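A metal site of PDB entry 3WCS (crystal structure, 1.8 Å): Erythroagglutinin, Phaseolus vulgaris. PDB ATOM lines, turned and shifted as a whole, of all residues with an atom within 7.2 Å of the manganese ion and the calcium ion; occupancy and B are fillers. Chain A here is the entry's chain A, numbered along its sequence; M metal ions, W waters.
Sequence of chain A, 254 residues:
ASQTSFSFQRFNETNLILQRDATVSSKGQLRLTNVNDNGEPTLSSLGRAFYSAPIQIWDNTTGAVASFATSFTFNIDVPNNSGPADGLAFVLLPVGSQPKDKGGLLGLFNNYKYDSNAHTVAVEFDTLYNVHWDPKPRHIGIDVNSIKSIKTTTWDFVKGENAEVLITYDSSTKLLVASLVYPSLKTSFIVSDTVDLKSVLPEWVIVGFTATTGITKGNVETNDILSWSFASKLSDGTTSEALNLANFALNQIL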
ATOM      1  N   ASP A  86     -19.720 -19.518  24.476  1.00  0.00           N
ATOM      2  CA  ASP A  86     -19.028 -19.940  23.228  1.00  0.00           C
ATOM      3  C   ASP A  86     -20.021 -20.312  22.142  1.00  0.00           C
ATOM      4  O   ASP A  86     -19.669 -20.383  20.943  1.00  0.00           O
ATOM      5  CB  ASP A  86     -18.167 -21.172  23.520  1.00  0.00           C
ATOM      6  CG  ASP A  86     -16.762 -20.816  23.880  1.00  0.00           C
ATOM      7  OD1 ASP A  86     -15.984 -20.491  22.941  1.00  0.00           O
ATOM      8  OD2 ASP A  86     -16.403 -20.905  25.081  1.00  0.00           O
ATOM      9  N   GLY A  87     -21.255 -20.628  22.548  1.00  0.00           N
ATOM     10  CA  GLY A  87     -22.320 -20.893  21.593  1.00  0.00           C
ATOM     11  C   GLY A  87     -23.138 -22.099  21.987  1.00  0.00           C
ATOM     12  O   GLY A  87     -22.954 -22.656  23.077  1.00  0.00           O
ATOM     13  N   GLY A 103     -15.884 -25.043  26.640  1.00  0.00           N
ATOM     14  CA  GLY A 103     -15.452 -23.872  25.857  1.00  0.00           C
ATOM     15  C   GLY A 103     -15.742 -23.992  24.359  1.00  0.00           C
ATOM     16  O   GLY A 103     -16.827 -24.379  23.943  1.00  0.00           O
ATOM     17  N   GLY A 104     -14.726 -23.682  23.538  1.00  0.00           N
ATOM     18  CA  GLY A 104     -14.925 -23.664  22.096  1.00  0.00           C
ATOM     19  C   GLY A 104     -15.203 -25.033  21.467  1.00  0.00           C
ATOM     20  O   GLY A 104     -15.582 -25.124  20.324  1.00  0.00           O
ATOM     21  N   LEU A 105     -14.989 -26.095  22.215  1.00  0.00           N
ATOM     22  CA  LEU A 105     -15.277 -27.426  21.697  1.00  0.00           C
ATOM     23  C   LEU A 105     -16.740 -27.846  21.954  1.00  0.00           C
ATOM     24  O   LEU A 105     -17.174 -28.928  21.525  1.00  0.00           O
ATOM     25  CB  LEU A 105     -14.281 -28.427  22.286  1.00  0.00           C
ATOM     26  CG  LEU A 105     -12.817 -28.135  21.874  1.00  0.00           C
ATOM     27  CD1 LEU A 105     -11.827 -29.020  22.629  1.00  0.00           C
ATOM     28  CD2 LEU A 105     -12.627 -28.221  20.365  1.00  0.00           C
ATOM     29  N   LEU A 106     -17.483 -26.976  22.631  1.00  0.00           N
ATOM     30  CA  LEU A 106     -18.961 -27.092  22.716  1.00  0.00           C
ATOM     31  C   LEU A 106     -19.501 -28.354  23.412  1.00  0.00           C
ATOM     32  O   LEU A 106     -20.685 -28.705  23.281  1.00  0.00           O
ATOM     33  CB  LEU A 106     -19.593 -26.914  21.324  1.00  0.00           C
ATOM     34  CG  LEU A 106     -19.361 -25.579  20.611  1.00  0.00           C
ATOM     35  CD1 LEU A 106     -20.060 -25.513  19.269  1.00  0.00           C
ATOM     36  CD2 LEU A 106     -19.761 -24.383  21.465  1.00  0.00           C
ATOM     37  N   GLU A 124     -24.185 -25.781  14.620  1.00  0.00           N
ATOM     38  CA  GLU A 124     -23.671 -24.889  15.653  1.00  0.00           C
ATOM     39  C   GLU A 124     -23.990 -23.428  15.405  1.00  0.00           C
ATOM     40  O   GLU A 124     -24.092 -22.986  14.255  1.00  0.00           O
ATOM     41  CB  GLU A 124     -22.159 -25.048  15.841  1.00  0.00           C
ATOM     42  CG  GLU A 124     -21.316 -24.662  14.600  1.00  0.00           C
ATOM     43  CD  GLU A 124     -19.826 -24.482  14.920  1.00  0.00           C
ATOM     44  OE1 GLU A 124     -19.255 -25.448  15.498  1.00  0.00           O
ATOM     45  OE2 GLU A 124     -19.201 -23.408  14.627  1.00  0.00           O
ATOM     46  N   PHE A 125     -24.227 -22.705  16.514  1.00  0.00           N
ATOM     47  CA  PHE A 125     -24.480 -21.275  16.518  1.00  0.00           C
ATOM     48  C   PHE A 125     -23.358 -20.729  17.368  1.00  0.00           C
ATOM     49  O   PHE A 125     -23.406 -20.775  18.590  1.00  0.00           O
ATOM     50  CB  PHE A 125     -25.911 -21.034  17.081  1.00  0.00           C
ATOM     51  CG  PHE A 125     -26.945 -21.660  16.212  1.00  0.00           C
ATOM     52  CD1 PHE A 125     -27.525 -20.948  15.167  1.00  0.00           C
ATOM     53  CD2 PHE A 125     -27.274 -23.016  16.362  1.00  0.00           C
ATOM     54  CE1 PHE A 125     -28.425 -21.535  14.309  1.00  0.00           C
ATOM     55  CE2 PHE A 125     -28.172 -23.614  15.495  1.00  0.00           C
ATOM     56  CZ  PHE A 125     -28.753 -22.886  14.488  1.00  0.00           C
ATOM     57  N   ASP A 126     -22.286 -20.323  16.680  1.00  0.00           N
ATOM     58  CA  ASP A 126     -20.940 -20.122  17.300  1.00  0.00           C
ATOM     59  C   ASP A 126     -20.706 -18.615  17.465  1.00  0.00           C
ATOM     60  O   ASP A 126     -20.691 -17.867  16.484  1.00  0.00           O
ATOM     61  CB  ASP A 126     -19.873 -20.780  16.373  1.00  0.00           C
ATOM     62  CG  ASP A 126     -18.451 -20.843  16.982  1.00  0.00           C
ATOM     63  OD1 ASP A 126     -18.229 -20.137  17.985  1.00  0.00           O
ATOM     64  OD2 ASP A 126     -17.554 -21.619  16.454  1.00  0.00           O
ATOM     65  N   THR A 127     -20.536 -18.188  18.724  1.00  0.00           N
ATOM     66  CA  THR A 127     -20.446 -16.770  19.057  1.00  0.00           C
ATOM     67  C   THR A 127     -19.052 -16.302  19.375  1.00  0.00           C
ATOM     68  O   THR A 127     -18.865 -15.119  19.726  1.00  0.00           O
ATOM     69  CB  THR A 127     -21.318 -16.455  20.296  1.00  0.00           C
ATOM     70  OG1 THR A 127     -20.864 -17.223  21.401  1.00  0.00           O
ATOM     71  CG2 THR A 127     -22.786 -16.759  19.988  1.00  0.00           C
ATOM     72  N   LEU A 128     -18.075 -17.206  19.287  1.00  0.00           N
ATOM     73  CA  LEU A 128     -16.688 -16.890  19.668  1.00  0.00           C
ATOM     74  C   LEU A 128     -15.711 -17.444  18.634  1.00  0.00           C
ATOM     75  O   LEU A 128     -15.657 -18.640  18.373  1.00  0.00           O
ATOM     76  CB  LEU A 128     -16.356 -17.445  21.058  1.00  0.00           C
ATOM     77  CG  LEU A 128     -14.957 -16.861  21.393  1.00  0.00           C
ATOM     78  CD1 LEU A 128     -14.883 -15.888  22.565  1.00  0.00           C
ATOM     79  CD2 LEU A 128     -13.828 -17.896  21.292  1.00  0.00           C
ATOM     80  N   TYR A 129     -14.918 -16.529  18.074  1.00  0.00           N
ATOM     81  CA  TYR A 129     -13.880 -16.907  17.085  1.00  0.00           C
ATOM     82  C   TYR A 129     -12.720 -17.659  17.730  1.00  0.00           C
ATOM     83  O   TYR A 129     -11.983 -17.093  18.557  1.00  0.00           O
ATOM     84  CB  TYR A 129     -13.395 -15.628  16.429  1.00  0.00           C
ATOM     85  CG  TYR A 129     -12.069 -15.733  15.676  1.00  0.00           C
ATOM     86  CD1 TYR A 129     -11.921 -16.618  14.637  1.00  0.00           C
ATOM     87  CD2 TYR A 129     -10.983 -14.963  16.060  1.00  0.00           C
ATOM     88  CE1 TYR A 129     -10.698 -16.688  13.944  1.00  0.00           C
ATOM     89  CE2 TYR A 129      -9.764 -15.025  15.390  1.00  0.00           C
ATOM     90  CZ  TYR A 129      -9.631 -15.892  14.345  1.00  0.00           C
ATOM     91  OH  TYR A 129      -8.402 -15.948  13.684  1.00  0.00           O
ATOM     92  N   ASN A 130     -12.549 -18.928  17.348  1.00  0.00           N
ATOM     93  CA  ASN A 130     -11.481 -19.754  17.888  1.00  0.00           C
ATOM     94  C   ASN A 130     -10.434 -19.806  16.789  1.00  0.00           C
ATOM     95  O   ASN A 130     -10.658 -20.379  15.733  1.00  0.00           O
ATOM     96  CB  ASN A 130     -11.991 -21.156  18.245  1.00  0.00           C
ATOM     97  CG  ASN A 130     -12.828 -21.162  19.519  1.00  0.00           C
ATOM     98  OD1 ASN A 130     -14.073 -21.246  19.471  1.00  0.00           O
ATOM     99  ND2 ASN A 130     -12.140 -21.088  20.665  1.00  0.00           N
ATOM    100  N   VAL A 131      -9.305 -19.154  17.045  1.00  0.00           N
ATOM    101  CA  VAL A 131      -8.287 -18.905  16.008  1.00  0.00           C
ATOM    102  C   VAL A 131      -7.820 -20.120  15.214  1.00  0.00           C
ATOM    103  O   VAL A 131      -7.480 -20.009  14.027  1.00  0.00           O
ATOM    104  CB  VAL A 131      -7.080 -18.145  16.638  1.00  0.00           C
ATOM    105  CG1 VAL A 131      -6.389 -18.988  17.703  1.00  0.00           C
ATOM    106  CG2 VAL A 131      -6.097 -17.698  15.569  1.00  0.00           C
ATOM    107  N   TRP A 133      -9.446 -22.810  14.213  1.00  0.00           N
ATOM    108  CA  TRP A 133     -10.406 -23.463  13.312  1.00  0.00           C
ATOM    109  C   TRP A 133     -11.566 -22.672  12.758  1.00  0.00           C
ATOM    110  O   TRP A 133     -12.118 -23.042  11.746  1.00  0.00           O
ATOM    111  CB  TRP A 133     -10.917 -24.769  13.933  1.00  0.00           C
ATOM    112  CG  TRP A 133     -11.793 -24.536  15.145  1.00  0.00           C
ATOM    113  CD1 TRP A 133     -13.142 -24.208  15.154  1.00  0.00           C
ATOM    114  CD2 TRP A 133     -11.413 -24.670  16.543  1.00  0.00           C
ATOM    115  NE1 TRP A 133     -13.605 -24.085  16.458  1.00  0.00           N
ATOM    116  CE2 TRP A 133     -12.621 -24.369  17.334  1.00  0.00           C
ATOM    117  CE3 TRP A 133     -10.231 -24.972  17.219  1.00  0.00           C
ATOM    118  CZ2 TRP A 133     -12.615 -24.389  18.708  1.00  0.00           C
ATOM    119  CZ3 TRP A 133     -10.239 -24.988  18.607  1.00  0.00           C
ATOM    120  CH2 TRP A 133     -11.409 -24.693  19.336  1.00  0.00           C
ATOM    121  N   ASP A 134     -11.986 -21.601  13.435  1.00  0.00           N
ATOM    122  CA  ASP A 134     -13.185 -20.854  13.029  1.00  0.00           C
ATOM    123  C   ASP A 134     -12.927 -19.757  11.983  1.00  0.00           C
ATOM    124  O   ASP A 134     -11.862 -19.156  11.997  1.00  0.00           O
ATOM    125  CB  ASP A 134     -13.794 -20.143  14.254  1.00  0.00           C
ATOM    126  CG  ASP A 134     -14.709 -21.056  15.098  1.00  0.00           C
ATOM    127  OD1 ASP A 134     -15.438 -21.955  14.561  1.00  0.00           O
ATOM    128  OD2 ASP A 134     -14.731 -20.783  16.332  1.00  0.00           O
ATOM    129  N   PRO A 135     -13.945 -19.442  11.137  1.00  0.00           N
ATOM    130  CA  PRO A 135     -13.972 -18.169  10.421  1.00  0.00           C
ATOM    131  C   PRO A 135     -14.117 -17.052  11.458  1.00  0.00           C
ATOM    132  O   PRO A 135     -14.664 -17.285  12.538  1.00  0.00           O
ATOM    133  CB  PRO A 135     -15.219 -18.267   9.538  1.00  0.00           C
ATOM    134  CG  PRO A 135     -16.101 -19.273  10.206  1.00  0.00           C
ATOM    135  CD  PRO A 135     -15.218 -20.203  10.981  1.00  0.00           C
ATOM    136  N   PRO A 137     -15.929 -14.063  11.486  1.00  0.00           N
ATOM    137  CA  PRO A 137     -17.289 -13.639  11.851  1.00  0.00           C
ATOM    138  C   PRO A 137     -18.031 -14.742  12.589  1.00  0.00           C
ATOM    139  O   PRO A 137     -17.823 -15.924  12.308  1.00  0.00           O
ATOM    140  CB  PRO A 137     -17.975 -13.369  10.511  1.00  0.00           C
ATOM    141  CG  PRO A 137     -16.836 -13.213   9.507  1.00  0.00           C
ATOM    142  CD  PRO A 137     -15.774 -14.139  10.011  1.00  0.00           C
ATOM    143  N   HIS A 139     -21.033 -17.236  13.304  1.00  0.00           N
ATOM    144  CA  HIS A 139     -21.452 -18.092  12.198  1.00  0.00           C
ATOM    145  C   HIS A 139     -22.381 -19.200  12.625  1.00  0.00           C
ATOM    146  O   HIS A 139     -22.393 -19.618  13.797  1.00  0.00           O
ATOM    147  CB  HIS A 139     -20.201 -18.693  11.489  1.00  0.00           C
ATOM    148  CG  HIS A 139     -19.233 -19.410  12.409  1.00  0.00           C
ATOM    149  ND1 HIS A 139     -18.300 -18.757  13.136  1.00  0.00           N
ATOM    150  CD2 HIS A 139     -19.127 -20.770  12.747  1.00  0.00           C
ATOM    151  CE1 HIS A 139     -17.595 -19.656  13.865  1.00  0.00           C
ATOM    152  NE2 HIS A 139     -18.109 -20.907  13.647  1.00  0.00           N
ATOM    153  N   ILE A 140     -23.167 -19.675  11.664  1.00  0.00           N
ATOM    154  CA  ILE A 140     -23.883 -20.940  11.828  1.00  0.00           C
ATOM    155  C   ILE A 140     -23.030 -21.932  11.065  1.00  0.00           C
ATOM    156  O   ILE A 140     -22.552 -21.612   9.976  1.00  0.00           O
ATOM    157  CB  ILE A 140     -25.284 -20.885  11.212  1.00  0.00           C
ATOM    158  CG1 ILE A 140     -26.081 -19.707  11.793  1.00  0.00           C
ATOM    159  CG2 ILE A 140     -26.015 -22.219  11.366  1.00  0.00           C
ATOM    160  CD1 ILE A 140     -27.251 -19.319  10.915  1.00  0.00           C
ATOM    161  N   GLY A 141     -22.765 -23.079  11.669  1.00  0.00           N
ATOM    162  CA  GLY A 141     -21.928 -24.102  10.999  1.00  0.00           C
ATOM    163  C   GLY A 141     -22.555 -25.487  11.054  1.00  0.00           C
ATOM    164  O   GLY A 141     -23.245 -25.822  12.014  1.00  0.00           O
ATOM    165  N   ASP A 143     -21.501 -29.250  11.451  1.00  0.00           N
ATOM    166  CA  ASP A 143     -20.372 -29.987  12.031  1.00  0.00           C
ATOM    167  C   ASP A 143     -20.586 -31.467  11.851  1.00  0.00           C
ATOM    168  O   ASP A 143     -21.597 -32.026  12.320  1.00  0.00           O
ATOM    169  CB  ASP A 143     -20.227 -29.706  13.540  1.00  0.00           C
ATOM    170  CG  ASP A 143     -19.858 -28.273  13.850  1.00  0.00           C
ATOM    171  OD1 ASP A 143     -19.655 -27.502  12.895  1.00  0.00           O
ATOM    172  OD2 ASP A 143     -19.799 -27.921  15.060  1.00  0.00           O
ATOM    173  N   ILE A 147     -15.067 -30.121  15.170  1.00  0.00           N
ATOM    174  CA  ILE A 147     -15.420 -28.726  15.490  1.00  0.00           C
ATOM    175  C   ILE A 147     -15.119 -27.800  14.301  1.00  0.00           C
ATOM    176  O   ILE A 147     -15.624 -26.678  14.232  1.00  0.00           O
ATOM    177  CB  ILE A 147     -14.749 -28.230  16.795  1.00  0.00           C
ATOM    178  CG1 ILE A 147     -15.467 -26.997  17.369  1.00  0.00           C
ATOM    179  CG2 ILE A 147     -13.283 -27.856  16.539  1.00  0.00           C
ATOM    180  CD1 ILE A 147     -16.872 -27.273  17.910  1.00  0.00           C
ATOM    181  N   LYS A 148     -14.278 -28.254  13.348  1.00  0.00           N
ATOM    182  CA  LYS A 148     -14.045 -27.481  12.131  1.00  0.00           C
ATOM    183  C   LYS A 148     -15.178 -27.746  11.163  1.00  0.00           C
ATOM    184  O   LYS A 148     -15.193 -28.802  10.487  1.00  0.00           O
ATOM    185  CB  LYS A 148     -12.684 -27.851  11.472  1.00  0.00           C
ATOM    186  CG  LYS A 148     -12.357 -26.970  10.280  1.00  0.00           C
ATOM    187  CD  LYS A 148     -11.268 -27.577   9.391  1.00  0.00           C
ATOM    188  CE  LYS A 148     -11.326 -26.926   8.024  1.00  0.00           C
ATOM    189  NZ  LYS A 148     -10.533 -27.651   6.978  1.00  0.00           N
ATOM    190  N   SER A 149     -16.118 -26.802  11.059  1.00  0.00           N
ATOM    191  CA  SER A 149     -17.386 -27.027  10.321  1.00  0.00           C
ATOM    192  C   SER A 149     -17.115 -27.361   8.878  1.00  0.00           C
ATOM    193  O   SER A 149     -16.222 -26.761   8.288  1.00  0.00           O
ATOM    194  CB  SER A 149     -18.266 -25.784  10.373  1.00  0.00           C
ATOM    195  OG  SER A 149     -18.523 -25.440  11.727  1.00  0.00           O
ATOM    196  N   THR A 152     -20.018 -23.133   6.644  1.00  0.00           N
ATOM    197  CA  THR A 152     -20.544 -22.063   7.519  1.00  0.00           C
ATOM    198  C   THR A 152     -21.199 -20.950   6.711  1.00  0.00           C
ATOM    199  O   THR A 152     -20.964 -20.814   5.511  1.00  0.00           O
ATOM    200  CB  THR A 152     -19.442 -21.438   8.414  1.00  0.00           C
ATOM    201  OG1 THR A 152     -18.413 -20.857   7.591  1.00  0.00           O
ATOM    202  CG2 THR A 152     -18.826 -22.474   9.380  1.00  0.00           C
HETATM  203 MN    MN M   1     -17.373 -22.521  14.634  1.00  0.00          MN
HETATM  204 CA    CA M   2     -16.045 -20.958  18.229  1.00  0.00          CA
HETATM  205  O   HOH W   1     -16.127 -23.286  18.067  1.00  0.00           O
HETATM  206  O   HOH W   2     -16.917 -24.197  15.551  1.00  0.00           O
HETATM  207  O   HOH W   3     -16.832 -23.377  12.909  1.00  0.00           O
HETATM  208  O   HOH W   4     -17.071 -20.981  20.295  1.00  0.00           O
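The indole nitrogen of Trp 133 sits close to the side-chain carboxylate of Asp 134 (3.4 Å). A ring nitrogen (ND1) of His 139 lies within hydrogen-bond range of the backbone carbonyl oxygen of Pro 137 (3.0 Å). The side-chain carboxylate of Asp 143 lies close to the side-chain carboxylate of Glu 124, 2.6 Å away. N of Glu 124 sits at hydrogen-bond distance from O of Gly 141 (2.8 Å).
The nearest printed residue that does not touch the manganese ion is Ser 149 (4.3 Å).
Within 4 Å of the calcium ion: Asp 126, Leu 128, Asn 130 and Asp 134. Along chain A the residues within 4 Å of the calcium ion span positions 126 to 134. The nearest printed residue that does not touch the calcium ion is Trp 133 (4.3 Å).
The manganese ion is bound by water W2, water W3, OD1 of Asp 134, NE2 of His 139, OE2 of Glu 124 and OD2 of Asp 126.
The calcium ion is bound by water W4 (2.3 Å), OD2 of Asp 134 (2.3 Å), water W1 (2.3 Å), OD1 of Asp 126 (2.3 Å), OD1 of Asn 130 (2.3 Å), O of Leu 128 (2.4 Å) and OD2 of Asp 126 (2.4 Å).
Water W2 lies within hydrogen-bond range of the side-chain carboxylate of Glu 124, the backbone carbonyl oxygen of Ile 147 and the indole nitrogen of Trp 133. Water W1 lies within hydrogen-bond range of O of Gly 104 (3.0 Å) and NE1 of Trp 133 (3.1 Å).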
